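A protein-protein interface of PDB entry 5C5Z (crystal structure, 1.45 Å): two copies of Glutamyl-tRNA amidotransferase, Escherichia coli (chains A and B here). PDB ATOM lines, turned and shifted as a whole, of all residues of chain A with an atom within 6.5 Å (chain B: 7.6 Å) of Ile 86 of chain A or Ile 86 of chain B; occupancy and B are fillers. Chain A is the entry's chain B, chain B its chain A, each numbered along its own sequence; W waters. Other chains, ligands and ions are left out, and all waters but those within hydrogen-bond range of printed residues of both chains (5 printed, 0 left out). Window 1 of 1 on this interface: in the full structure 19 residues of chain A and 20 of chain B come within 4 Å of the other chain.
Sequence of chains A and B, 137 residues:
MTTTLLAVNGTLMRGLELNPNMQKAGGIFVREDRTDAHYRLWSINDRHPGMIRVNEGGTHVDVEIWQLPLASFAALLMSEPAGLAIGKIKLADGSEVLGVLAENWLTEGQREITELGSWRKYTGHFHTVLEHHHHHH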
ATOM      1  N   LEU A   6      18.021  11.917 -17.696  1.00  0.00           N
ATOM      2  CA  LEU A   6      17.825  11.552 -19.098  1.00  0.00           C
ATOM      3  C   LEU A   6      17.541  10.063 -19.211  1.00  0.00           C
ATOM      4  O   LEU A   6      18.260   9.257 -18.629  1.00  0.00           O
ATOM      5  CB  LEU A   6      19.081  11.895 -19.910  1.00  0.00           C
ATOM      6  CG  LEU A   6      19.017  11.546 -21.404  1.00  0.00           C
ATOM      7  CD1 LEU A   6      17.983  12.374 -22.115  1.00  0.00           C
ATOM      8  CD2 LEU A   6      20.385  11.726 -22.054  1.00  0.00           C
ATOM      9  N   PHE A  73      24.656  18.078 -21.704  1.00  0.00           N
ATOM     10  CA  PHE A  73      23.659  17.659 -22.690  1.00  0.00           C
ATOM     11  C   PHE A  73      24.004  17.998 -24.138  1.00  0.00           C
ATOM     12  O   PHE A  73      23.799  17.172 -25.013  1.00  0.00           O
ATOM     13  CB  PHE A  73      22.277  18.214 -22.337  1.00  0.00           C
ATOM     14  CG  PHE A  73      21.582  17.452 -21.257  1.00  0.00           C
ATOM     15  CD1 PHE A  73      21.928  17.627 -19.924  1.00  0.00           C
ATOM     16  CD2 PHE A  73      20.595  16.523 -21.573  1.00  0.00           C
ATOM     17  CE1 PHE A  73      21.287  16.907 -18.924  1.00  0.00           C
ATOM     18  CE2 PHE A  73      19.954  15.808 -20.577  1.00  0.00           C
ATOM     19  CZ  PHE A  73      20.304  15.993 -19.255  1.00  0.00           C
ATOM     20  N   LEU A  76      26.758  15.682 -25.515  1.00  0.00           N
ATOM     21  CA  LEU A  76      26.288  14.307 -25.582  1.00  0.00           C
ATOM     22  C   LEU A  76      25.390  14.145 -26.803  1.00  0.00           C
ATOM     23  O   LEU A  76      25.544  13.195 -27.575  1.00  0.00           O
ATOM     24  CB  LEU A  76      25.558  13.924 -24.293  1.00  0.00           C
ATOM     25  CG  LEU A  76      25.150  12.456 -24.181  1.00  0.00           C
ATOM     26  CD1 LEU A  76      26.375  11.578 -24.103  1.00  0.00           C
ATOM     27  CD2 LEU A  76      24.235  12.242 -22.975  1.00  0.00           C
ATOM     28  N   LEU A  77      24.476  15.090 -27.004  1.00  0.00           N
ATOM     29  CA  LEU A  77      23.587  15.055 -28.159  1.00  0.00           C
ATOM     30  C   LEU A  77      24.371  15.132 -29.466  1.00  0.00           C
ATOM     31  O   LEU A  77      24.109  14.378 -30.401  1.00  0.00           O
ATOM     32  CB  LEU A  77      22.568  16.190 -28.066  1.00  0.00           C
ATOM     33  CG  LEU A  77      21.575  16.327 -29.214  1.00  0.00           C
ATOM     34  CD1 LEU A  77      20.849  14.990 -29.493  1.00  0.00           C
ATOM     35  CD2 LEU A  77      20.588  17.429 -28.902  1.00  0.00           C
ATOM     36  N   GLU A  80      25.709  11.905 -30.544  1.00  0.00           N
ATOM     37  CA  GLU A  80      24.721  10.863 -30.814  1.00  0.00           C
ATOM     38  C   GLU A  80      24.611  10.530 -32.303  1.00  0.00           C
ATOM     39  O   GLU A  80      24.935  11.357 -33.141  1.00  0.00           O
ATOM     40  CB  GLU A  80      23.354  11.291 -30.263  1.00  0.00           C
ATOM     41  CG  GLU A  80      23.213  11.053 -28.772  1.00  0.00           C
ATOM     42  CD  GLU A  80      23.180   9.580 -28.444  1.00  0.00           C
ATOM     43  OE1 GLU A  80      24.250   9.001 -28.174  1.00  0.00           O
ATOM     44  OE2 GLU A  80      22.072   9.007 -28.472  1.00  0.00           O
ATOM     45  N   LEU A  84      18.718  11.319 -34.074  1.00  0.00           N
ATOM     46  CA  LEU A  84      18.269  11.261 -32.686  1.00  0.00           C
ATOM     47  C   LEU A  84      18.197  12.663 -32.084  1.00  0.00           C
ATOM     48  O   LEU A  84      18.967  13.550 -32.457  1.00  0.00           O
ATOM     49  CB  LEU A  84      19.193  10.382 -31.845  1.00  0.00           C
ATOM     50  CG  LEU A  84      19.252   8.913 -32.275  1.00  0.00           C
ATOM     51  CD1 LEU A  84      20.113   8.133 -31.296  1.00  0.00           C
ATOM     52  CD2 LEU A  84      17.855   8.304 -32.356  1.00  0.00           C
ATOM     53  N   ALA A  85      17.250  12.846 -31.167  1.00  0.00           N
ATOM     54  CA  ALA A  85      16.982  14.147 -30.559  1.00  0.00           C
ATOM     55  C   ALA A  85      16.679  13.917 -29.082  1.00  0.00           C
ATOM     56  O   ALA A  85      16.480  12.777 -28.660  1.00  0.00           O
ATOM     57  CB  ALA A  85      15.780  14.796 -31.255  1.00  0.00           C
ATOM     58  N   ILE A  86      16.641  14.982 -28.292  1.00  0.00           N
ATOM     59  CA  ILE A  86      16.238  14.864 -26.891  1.00  0.00           C
ATOM     60  C   ILE A  86      14.997  15.713 -26.664  1.00  0.00           C
ATOM     61  O   ILE A  86      14.963  16.890 -27.025  1.00  0.00           O
ATOM     62  CB  ILE A  86      17.354  15.306 -25.917  1.00  0.00           C
ATOM     63  CG1 ILE A  86      18.562  14.378 -26.057  1.00  0.00           C
ATOM     64  CG2 ILE A  86      16.830  15.319 -24.479  1.00  0.00           C
ATOM     65  CD1 ILE A  86      19.755  14.797 -25.246  1.00  0.00           C
ATOM     66  N   GLY A  87      13.961  15.103 -26.098  1.00  0.00           N
ATOM     67  CA  GLY A  87      12.750  15.821 -25.729  1.00  0.00           C
ATOM     68  C   GLY A  87      12.171  15.261 -24.456  1.00  0.00           C
ATOM     69  O   GLY A  87      12.879  14.608 -23.702  1.00  0.00           O
ATOM     70  N   LYS A  88      10.892  15.506 -24.206  1.00  0.00           N
ATOM     71  CA  LYS A  88      10.248  14.996 -23.002  1.00  0.00           C
ATOM     72  C   LYS A  88       9.507  13.700 -23.290  1.00  0.00           C
ATOM     73  O   LYS A  88       8.820  13.590 -24.306  1.00  0.00           O
ATOM     74  CB  LYS A  88       9.295  16.043 -22.430  1.00  0.00           C
ATOM     75  CG  LYS A  88      10.035  17.211 -21.806  1.00  0.00           C
ATOM     76  CD  LYS A  88       9.111  18.371 -21.456  1.00  0.00           C
ATOM     77  CE  LYS A  88       9.910  19.490 -20.786  1.00  0.00           C
ATOM     78  NZ  LYS A  88       9.042  20.668 -20.471  1.00  0.00           N
ATOM     79  N   LEU A  98      13.331  13.872 -19.445  1.00  0.00           N
ATOM     80  CA  LEU A  98      13.930  14.003 -20.764  1.00  0.00           C
ATOM     81  C   LEU A  98      14.306  12.620 -21.280  1.00  0.00           C
ATOM     82  O   LEU A  98      14.679  11.750 -20.512  1.00  0.00           O
ATOM     83  CB  LEU A  98      15.172  14.885 -20.724  1.00  0.00           C
ATOM     84  CG  LEU A  98      14.941  16.342 -20.332  1.00  0.00           C
ATOM     85  CD1 LEU A  98      16.276  17.068 -20.321  1.00  0.00           C
ATOM     86  CD2 LEU A  98      13.964  17.028 -21.294  1.00  0.00           C
ATOM     87  N   GLY A  99      14.222  12.422 -22.588  1.00  0.00           N
ATOM     88  CA  GLY A  99      14.596  11.151 -23.179  1.00  0.00           C
ATOM     89  C   GLY A  99      15.051  11.291 -24.614  1.00  0.00           C
ATOM     90  O   GLY A  99      14.717  12.265 -25.298  1.00  0.00           O
ATOM     91  N   VAL A 100      15.811  10.298 -25.066  1.00  0.00           N
ATOM     92  CA  VAL A 100      16.293  10.248 -26.436  1.00  0.00           C
ATOM     93  C   VAL A 100      15.219   9.677 -27.365  1.00  0.00           C
ATOM     94  O   VAL A 100      14.686   8.581 -27.138  1.00  0.00           O
ATOM     95  CB  VAL A 100      17.577   9.406 -26.549  1.00  0.00           C
ATOM     96  CG1 VAL A 100      18.038   9.358 -27.992  1.00  0.00           C
ATOM     97  CG2 VAL A 100      18.683   9.985 -25.642  1.00  0.00           C
ATOM     98  N   LEU A 101      14.918  10.443 -28.409  1.00  0.00           N
ATOM     99  CA  LEU A 101      13.852  10.164 -29.362  1.00  0.00           C
ATOM    100  C   LEU A 101      14.425  10.111 -30.761  1.00  0.00           C
ATOM    101  O   LEU A 101      15.472  10.705 -31.028  1.00  0.00           O
ATOM    102  CB  LEU A 101      12.820  11.289 -29.323  1.00  0.00           C
ATOM    103  CG  LEU A 101      12.021  11.427 -28.030  1.00  0.00           C
ATOM    104  CD1 LEU A 101      11.326  12.776 -27.947  1.00  0.00           C
ATOM    105  CD2 LEU A 101      11.013  10.292 -27.906  1.00  0.00           C
ATOM    106  N   LEU B   5      25.598  26.295 -30.348  1.00  0.00           N
ATOM    107  CA  LEU B   5      24.732  27.052 -31.241  1.00  0.00           C
ATOM    108  C   LEU B   5      23.404  26.340 -31.418  1.00  0.00           C
ATOM    109  O   LEU B   5      23.344  25.104 -31.475  1.00  0.00           O
ATOM    110  CB  LEU B   5      25.401  27.242 -32.599  1.00  0.00           C
ATOM    111  CG  LEU B   5      26.666  28.093 -32.498  1.00  0.00           C
ATOM    112  CD1 LEU B   5      27.507  27.972 -33.758  1.00  0.00           C
ATOM    113  CD2 LEU B   5      26.327  29.546 -32.235  1.00  0.00           C
ATOM    114  N   LEU B   6      22.336  27.121 -31.502  1.00  0.00           N
ATOM    115  CA  LEU B   6      20.994  26.562 -31.619  1.00  0.00           C
ATOM    116  C   LEU B   6      20.174  27.366 -32.606  1.00  0.00           C
ATOM    117  O   LEU B   6      20.138  28.602 -32.531  1.00  0.00           O
ATOM    118  CB  LEU B   6      20.304  26.567 -30.247  1.00  0.00           C
ATOM    119  CG  LEU B   6      18.870  26.025 -30.228  1.00  0.00           C
ATOM    120  CD1 LEU B   6      18.839  24.521 -30.473  1.00  0.00           C
ATOM    121  CD2 LEU B   6      18.209  26.345 -28.905  1.00  0.00           C
ATOM    122  N   ALA B   7      19.519  26.658 -33.527  1.00  0.00           N
ATOM    123  CA  ALA B   7      18.574  27.267 -34.458  1.00  0.00           C
ATOM    124  C   ALA B   7      17.182  27.245 -33.854  1.00  0.00           C
ATOM    125  O   ALA B   7      16.641  26.173 -33.566  1.00  0.00           O
ATOM    126  CB  ALA B   7      18.575  26.531 -35.789  1.00  0.00           C
ATOM    127  N   VAL B   8      16.614  28.436 -33.654  1.00  0.00           N
ATOM    128  CA  VAL B   8      15.251  28.571 -33.138  1.00  0.00           C
ATOM    129  C   VAL B   8      14.348  29.186 -34.204  1.00  0.00           C
ATOM    130  O   VAL B   8      14.817  29.968 -35.038  1.00  0.00           O
ATOM    131  CB  VAL B   8      15.211  29.398 -31.827  1.00  0.00           C
ATOM    132  CG1 VAL B   8      16.106  28.751 -30.763  1.00  0.00           C
ATOM    133  CG2 VAL B   8      15.630  30.859 -32.069  1.00  0.00           C
ATOM    134  N   LEU B  12      11.307  32.088 -29.244  1.00  0.00           N
ATOM    135  CA  LEU B  12      12.625  32.408 -28.684  1.00  0.00           C
ATOM    136  C   LEU B  12      13.350  33.471 -29.508  1.00  0.00           C
ATOM    137  O   LEU B  12      14.369  34.018 -29.079  1.00  0.00           O
ATOM    138  CB  LEU B  12      13.496  31.150 -28.597  1.00  0.00           C
ATOM    139  CG  LEU B  12      13.101  30.129 -27.532  1.00  0.00           C
ATOM    140  CD1 LEU B  12      13.727  28.775 -27.825  1.00  0.00           C
ATOM    141  CD2 LEU B  12      13.506  30.629 -26.160  1.00  0.00           C
ATOM    142  N   LEU B  68      24.508  29.947 -26.994  1.00  0.00           N
ATOM    143  CA  LEU B  68      24.177  29.965 -25.577  1.00  0.00           C
ATOM    144  C   LEU B  68      25.047  29.051 -24.734  1.00  0.00           C
ATOM    145  O   LEU B  68      25.601  28.067 -25.229  1.00  0.00           O
ATOM    146  CB  LEU B  68      22.686  29.738 -25.353  1.00  0.00           C
ATOM    147  CG  LEU B  68      22.154  28.321 -25.456  1.00  0.00           C
ATOM    148  CD1 LEU B  68      20.660  28.352 -25.120  1.00  0.00           C
ATOM    149  CD2 LEU B  68      22.359  27.706 -26.823  1.00  0.00           C
ATOM    150  N   SER B  72      22.542  26.486 -20.246  1.00  0.00           N
ATOM    151  CA  SER B  72      21.321  27.148 -20.707  1.00  0.00           C
ATOM    152  C   SER B  72      20.627  26.331 -21.792  1.00  0.00           C
ATOM    153  O   SER B  72      19.405  26.348 -21.921  1.00  0.00           O
ATOM    154  CB  SER B  72      21.629  28.558 -21.209  1.00  0.00           C
ATOM    155  OG  SER B  72      22.147  29.332 -20.155  1.00  0.00           O
ATOM    156  N   PHE B  73      21.420  25.609 -22.571  1.00  0.00           N
ATOM    157  CA  PHE B  73      20.876  24.691 -23.555  1.00  0.00           C
ATOM    158  C   PHE B  73      20.017  23.608 -22.874  1.00  0.00           C
ATOM    159  O   PHE B  73      18.876  23.336 -23.283  1.00  0.00           O
ATOM    160  CB  PHE B  73      22.036  24.083 -24.337  1.00  0.00           C
ATOM    161  CG  PHE B  73      21.620  23.029 -25.301  1.00  0.00           C
ATOM    162  CD1 PHE B  73      21.616  21.692 -24.927  1.00  0.00           C
ATOM    163  CD2 PHE B  73      21.230  23.365 -26.588  1.00  0.00           C
ATOM    164  CE1 PHE B  73      21.224  20.714 -25.815  1.00  0.00           C
ATOM    165  CE2 PHE B  73      20.836  22.383 -27.478  1.00  0.00           C
ATOM    166  CZ  PHE B  73      20.831  21.058 -27.092  1.00  0.00           C
ATOM    167  N   ALA B  74      20.549  23.000 -21.818  1.00  0.00           N
ATOM    168  CA  ALA B  74      19.785  22.020 -21.054  1.00  0.00           C
ATOM    169  C   ALA B  74      18.550  22.632 -20.379  1.00  0.00           C
ATOM    170  O   ALA B  74      17.504  21.977 -20.270  1.00  0.00           O
ATOM    171  CB  ALA B  74      20.670  21.333 -20.025  1.00  0.00           C
ATOM    172  N   ALA B  75      18.668  23.877 -19.914  1.00  0.00           N
ATOM    173  CA  ALA B  75      17.525  24.562 -19.314  1.00  0.00           C
ATOM    174  C   ALA B  75      16.377  24.680 -20.314  1.00  0.00           C
ATOM    175  O   ALA B  75      15.211  24.568 -19.945  1.00  0.00           O
ATOM    176  CB  ALA B  75      17.939  25.939 -18.791  1.00  0.00           C
ATOM    177  N   LEU B  76      16.707  24.893 -21.583  1.00  0.00           N
ATOM    178  CA  LEU B  76      15.693  24.946 -22.627  1.00  0.00           C
ATOM    179  C   LEU B  76      15.058  23.570 -22.882  1.00  0.00           C
ATOM    180  O   LEU B  76      13.856  23.467 -23.095  1.00  0.00           O
ATOM    181  CB  LEU B  76      16.279  25.521 -23.919  1.00  0.00           C
ATOM    182  CG  LEU B  76      15.247  25.656 -25.029  1.00  0.00           C
ATOM    183  CD1 LEU B  76      14.103  26.584 -24.597  1.00  0.00           C
ATOM    184  CD2 LEU B  76      15.889  26.148 -26.303  1.00  0.00           C
ATOM    185  N   LEU B  77      15.859  22.508 -22.853  1.00  0.00           N
ATOM    186  CA  LEU B  77      15.292  21.159 -22.938  1.00  0.00           C
ATOM    187  C   LEU B  77      14.247  20.952 -21.848  1.00  0.00           C
ATOM    188  O   LEU B  77      13.207  20.333 -22.076  1.00  0.00           O
ATOM    189  CB  LEU B  77      16.376  20.095 -22.803  1.00  0.00           C
ATOM    190  CG  LEU B  77      17.318  19.884 -23.982  1.00  0.00           C
ATOM    191  CD1 LEU B  77      18.449  18.943 -23.594  1.00  0.00           C
ATOM    192  CD2 LEU B  77      16.556  19.342 -25.184  1.00  0.00           C
ATOM    193  N   MET B  78      14.526  21.485 -20.662  1.00  0.00           N
ATOM    194  CA  MET B  78      13.613  21.336 -19.535  1.00  0.00           C
ATOM    195  C   MET B  78      12.377  22.220 -19.621  1.00  0.00           C
ATOM    196  O   MET B  78      11.302  21.824 -19.181  1.00  0.00           O
ATOM    197  CB  MET B  78      14.346  21.614 -18.226  1.00  0.00           C
ATOM    198  CG  MET B  78      15.453  20.616 -17.918  1.00  0.00           C
ATOM    199  SD  MET B  78      16.387  20.999 -16.270  1.00  0.00           S
ATOM    200  CE  MET B  78      14.856  21.211 -15.088  1.00  0.00           C
ATOM    201  N   GLU B  80      11.055  23.840 -22.535  1.00  0.00           N
ATOM    202  CA  GLU B  80      10.262  23.819 -23.765  1.00  0.00           C
ATOM    203  C   GLU B  80       9.099  22.840 -23.624  1.00  0.00           C
ATOM    204  O   GLU B  80       9.237  21.781 -23.009  1.00  0.00           O
ATOM    205  CB  GLU B  80      11.133  23.502 -24.990  1.00  0.00           C
ATOM    206  CG  GLU B  80      11.653  22.063 -25.058  1.00  0.00           C
ATOM    207  CD  GLU B  80      12.630  21.837 -26.209  1.00  0.00           C
ATOM    208  OE1 GLU B  80      12.859  22.769 -27.005  1.00  0.00           O
ATOM    209  OE2 GLU B  80      13.184  20.717 -26.307  1.00  0.00           O
ATOM    210  N   LEU B  84       8.122  19.335 -28.201  1.00  0.00           N
ATOM    211  CA  LEU B  84       9.307  19.929 -28.819  1.00  0.00           C
ATOM    212  C   LEU B  84      10.534  19.160 -28.344  1.00  0.00           C
ATOM    213  O   LEU B  84      10.559  18.631 -27.231  1.00  0.00           O
ATOM    214  CB  LEU B  84       9.445  21.419 -28.481  1.00  0.00           C
ATOM    215  CG  LEU B  84       8.355  22.347 -29.040  1.00  0.00           C
ATOM    216  CD1 LEU B  84       8.642  23.805 -28.689  1.00  0.00           C
ATOM    217  CD2 LEU B  84       8.198  22.193 -30.545  1.00  0.00           C
ATOM    218  N   ALA B  85      11.540  19.073 -29.201  1.00  0.00           N
ATOM    219  CA  ALA B  85      12.754  18.339 -28.885  1.00  0.00           C
ATOM    220  C   ALA B  85      13.897  19.042 -29.588  1.00  0.00           C
ATOM    221  O   ALA B  85      13.672  19.794 -30.533  1.00  0.00           O
ATOM    222  CB  ALA B  85      12.634  16.896 -29.374  1.00  0.00           C
ATOM    223  N   ILE B  86      15.126  18.797 -29.161  1.00  0.00           N
ATOM    224  CA  ILE B  86      16.271  19.365 -29.865  1.00  0.00           C
ATOM    225  C   ILE B  86      17.055  18.252 -30.541  1.00  0.00           C
ATOM    226  O   ILE B  86      17.382  17.238 -29.921  1.00  0.00           O
ATOM    227  CB  ILE B  86      17.170  20.212 -28.943  1.00  0.00           C
ATOM    228  CG1 ILE B  86      16.358  21.375 -28.361  1.00  0.00           C
ATOM    229  CG2 ILE B  86      18.367  20.732 -29.714  1.00  0.00           C
ATOM    230  CD1 ILE B  86      17.128  22.273 -27.387  1.00  0.00           C
ATOM    231  N   GLY B  87      17.313  18.439 -31.832  1.00  0.00           N
ATOM    232  CA  GLY B  87      18.111  17.514 -32.609  1.00  0.00           C
ATOM    233  C   GLY B  87      19.020  18.269 -33.544  1.00  0.00           C
ATOM    234  O   GLY B  87      19.287  19.449 -33.337  1.00  0.00           O
ATOM    235  N   LYS B  88      19.498  17.588 -34.574  1.00  0.00           N
ATOM    236  CA  LYS B  88      20.368  18.216 -35.551  1.00  0.00           C
ATOM    237  C   LYS B  88      19.576  18.611 -36.776  1.00  0.00           C
ATOM    238  O   LYS B  88      18.793  17.819 -37.296  1.00  0.00           O
ATOM    239  CB  LYS B  88      21.500  17.267 -35.936  1.00  0.00           C
ATOM    240  CG  LYS B  88      22.437  16.996 -34.780  1.00  0.00           C
ATOM    241  CD  LYS B  88      23.111  15.648 -34.932  1.00  0.00           C
ATOM    242  CE  LYS B  88      24.066  15.405 -33.776  1.00  0.00           C
ATOM    243  NZ  LYS B  88      24.326  13.936 -33.582  1.00  0.00           N
ATOM    244  N   ILE B  89      19.765  19.842 -37.236  1.00  0.00           N
ATOM    245  CA  ILE B  89      19.115  20.259 -38.466  1.00  0.00           C
ATOM    246  C   ILE B  89      20.144  20.649 -39.505  1.00  0.00           C
ATOM    247  O   ILE B  89      21.321  20.836 -39.185  1.00  0.00           O
ATOM    248  CB  ILE B  89      18.111  21.403 -38.247  1.00  0.00           C
ATOM    249  CG1 ILE B  89      18.829  22.703 -37.903  1.00  0.00           C
ATOM    250  CG2 ILE B  89      17.085  21.021 -37.158  1.00  0.00           C
ATOM    251  CD1 ILE B  89      17.958  23.915 -38.139  1.00  0.00           C
ATOM    252  N   VAL B  97      23.510  22.235 -37.590  1.00  0.00           N
ATOM    253  CA  VAL B  97      23.484  22.926 -36.307  1.00  0.00           C
ATOM    254  C   VAL B  97      22.383  22.285 -35.463  1.00  0.00           C
ATOM    255  O   VAL B  97      21.442  21.725 -36.016  1.00  0.00           O
ATOM    256  CB  VAL B  97      23.224  24.448 -36.498  1.00  0.00           C
ATOM    257  CG1 VAL B  97      21.827  24.701 -37.042  1.00  0.00           C
ATOM    258  CG2 VAL B  97      23.445  25.208 -35.195  1.00  0.00           C
ATOM    259  N   LEU B  98      22.492  22.345 -34.141  1.00  0.00           N
ATOM    260  CA  LEU B  98      21.394  21.895 -33.299  1.00  0.00           C
ATOM    261  C   LEU B  98      20.191  22.800 -33.546  1.00  0.00           C
ATOM    262  O   LEU B  98      20.347  23.993 -33.816  1.00  0.00           O
ATOM    263  CB  LEU B  98      21.784  21.913 -31.817  1.00  0.00           C
ATOM    264  CG  LEU B  98      22.879  20.913 -31.431  1.00  0.00           C
ATOM    265  CD1 LEU B  98      23.309  21.112 -29.973  1.00  0.00           C
ATOM    266  CD2 LEU B  98      22.400  19.477 -31.672  1.00  0.00           C
ATOM    267  N   GLY B  99      18.990  22.231 -33.481  1.00  0.00           N
ATOM    268  CA  GLY B  99      17.782  23.003 -33.719  1.00  0.00           C
ATOM    269  C   GLY B  99      16.574  22.384 -33.049  1.00  0.00           C
ATOM    270  O   GLY B  99      16.521  21.174 -32.821  1.00  0.00           O
ATOM    271  N   VAL B 100      15.588  23.218 -32.740  1.00  0.00           N
ATOM    272  CA  VAL B 100      14.362  22.742 -32.114  1.00  0.00           C
ATOM    273  C   VAL B 100      13.414  22.161 -33.153  1.00  0.00           C
ATOM    274  O   VAL B 100      13.124  22.793 -34.174  1.00  0.00           O
ATOM    275  CB  VAL B 100      13.648  23.866 -31.338  1.00  0.00           C
ATOM    276  CG1 VAL B 100      12.461  23.308 -30.574  1.00  0.00           C
ATOM    277  CG2 VAL B 100      14.616  24.565 -30.387  1.00  0.00           C
ATOM    278  N   LEU B 101      12.958  20.945 -32.876  1.00  0.00           N
ATOM    279  CA  LEU B 101      12.072  20.181 -33.750  1.00  0.00           C
ATOM    280  C   LEU B 101      10.784  19.865 -33.000  1.00  0.00           C
ATOM    281  O   LEU B 101      10.726  19.985 -31.776  1.00  0.00           O
ATOM    282  CB  LEU B 101      12.752  18.867 -34.117  1.00  0.00           C
ATOM    283  CG  LEU B 101      14.064  18.961 -34.884  1.00  0.00           C
ATOM    284  CD1 LEU B 101      14.802  17.608 -34.849  1.00  0.00           C
ATOM    285  CD2 LEU B 101      13.807  19.409 -36.314  1.00  0.00           C
ATOM    286  N   ALA B 102       9.756  19.454 -33.738  1.00  0.00           N
ATOM    287  CA  ALA B 102       8.550  18.892 -33.136  1.00  0.00           C
ATOM    288  C   ALA B 102       8.516  17.382 -33.312  1.00  0.00           C
ATOM    289  O   ALA B 102       8.945  16.861 -34.345  1.00  0.00           O
ATOM    290  CB  ALA B 102       7.295  19.502 -33.774  1.00  0.00           C
ATOM    291  N   GLU B 103       8.001  16.689 -32.299  1.00  0.00           N
ATOM    292  CA  GLU B 103       7.597  15.293 -32.445  1.00  0.00           C
ATOM    293  C   GLU B 103       6.349  15.210 -33.323  1.00  0.00           C
ATOM    294  O   GLU B 103       5.497  16.108 -33.300  1.00  0.00           O
ATOM    295  CB  GLU B 103       7.260  14.712 -31.078  1.00  0.00           C
ATOM    296  CG  GLU B 103       8.438  14.555 -30.120  1.00  0.00           C
ATOM    297  CD  GLU B 103       7.989  14.031 -28.776  1.00  0.00           C
ATOM    298  OE1 GLU B 103       7.807  12.807 -28.645  1.00  0.00           O
ATOM    299  OE2 GLU B 103       7.757  14.849 -27.864  1.00  0.00           O
HETATM  300  O   HOH W   1       6.591  14.861 -25.327  1.00  0.00           O
HETATM  301  O   HOH W   2       7.993  11.712 -26.150  1.00  0.00           O
HETATM  302  O   HOH W   3      21.832  12.914 -32.863  1.00  0.00           O
HETATM  303  O   HOH W   4      18.542  14.928 -34.816  1.00  0.00           O
HETATM  304  O   HOH W   5       9.221  16.484 -26.298  1.00  0.00           O
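NZ of Lys 88 of chain A is in hydrogen-bond range of O of Met 78 of chain B, 2.8 Å away. NZ of Lys 88 of chain A is in hydrogen-bond range of O of Glu 80 of chain B, at 2.8 Å. The backbone NH (N) of Ile 86 of chain B is in hydrogen-bond range of the backbone carbonyl oxygen (O) of Ile 86 of chain A (2.9 Å). NZ of Lys 88 of chain B sits at hydrogen-bond distance from O of Leu 77 of chain A. NZ of Lys 88 of chain B sits at hydrogen-bond distance from O of Glu 80 of chain A, 2.7 Å away.
O of Ala 85 of chain B sits at hydrogen-bond distance from N of Leu 101 of chain B (2.7 Å). The backbone carbonyl oxygen (O) of Leu 101 of chain A sits at hydrogen-bond distance from the backbone NH (N) of Ala 85 of chain A (2.8 Å). O of Gly 87 of chain A is in hydrogen-bond range of N of Gly 99 of chain A (2.8 Å).
O of Ile 86 of chain A touches CD2 of Leu 77 of chain B (3.5 Å). Ile 86 of chain A touches Ala 85 of chain B (O to CA, 3.2 Å). Leu 84 of chain B touches Gly 87 of chain A (O to CA, 3.9 Å). O of Leu 77 of chain B touches CE of Lys 88 of chain A (3.6 Å). Leu 98 of chain A touches Leu 77 of chain B.
Printed residues of chain A within 4 Å of Ile 86 of chain B: Leu 77 (3.4 Å), Ala 85 (3.2 Å) and Ile 86 (2.9 Å). Of the printed residues of chain A, Ala 85 of chain B touches Ile 86 (3.2 Å) and Gly 87 (3.8 Å). Of the printed residues of chain A, Leu 98 of chain B touches Leu 77. Printed residues of chain A within 4 Å of Glu 80 of chain B: Lys 88. The nearest residue of chain B that does not touch Ile 86 of chain A is Glu 80 of chain B (4.3 Å).
Of the 14 printed residues of chain A, 9 touch a printed residue of chain B. Printed residues of chain A that touch a printed residue of chain B: Phe 73, Leu 77, Glu 80, Ala 85, Ile 86, Gly 87, Lys 88, Leu 98 and Leu 101. Hydrophobic or aromatic side chains of chain A within 4 Å of the printed part of chain B: Phe 73, Leu 77, Ala 85, Leu 98 and Leu 101. Of the 27 printed residues of chain B, 11 touch a printed residue of chain A. Hydrophobic or aromatic side chains of chain B within 4 Å of the printed part of chain A: Ala 74, Leu 77, Ala 85 and Leu 98. Along chain B the printed residues that touch a printed residue of chain A span positions 74 to 103. Among the printed residues, no Asp or Glu carboxylate lies within 4 Å of a Lys or Arg side-chain nitrogen of the other chain.
Glu 80 of chain A touches Lys 88 of chain B, and with the chains exchanged Lys 88 of chain A touches Glu 80 of chain B. Ala 85 of chain A touches Gly 87 of chain B, and with the chains exchanged Gly 87 of chain A touches Ala 85 of chain B. Ile 86 of chain A touches its own counterpart, Ile 86 of chain B. 14 positions are printed for both chains.
Water W4 bridges the backbone carbonyl oxygen of Leu 84 of chain A (2.8 Å) and the backbone NH of Lys 88 of chain B (2.8 Å). Water W3 lies within hydrogen-bond range of the side-chain amino group (NZ) of Lys 88 of chain B (2.8 Å), the backbone carbonyl oxygen (O) of Leu 84 of chain A (3.0 Å) and the backbone carbonyl oxygen (O) of Glu 80 of chain A (3.5 Å).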
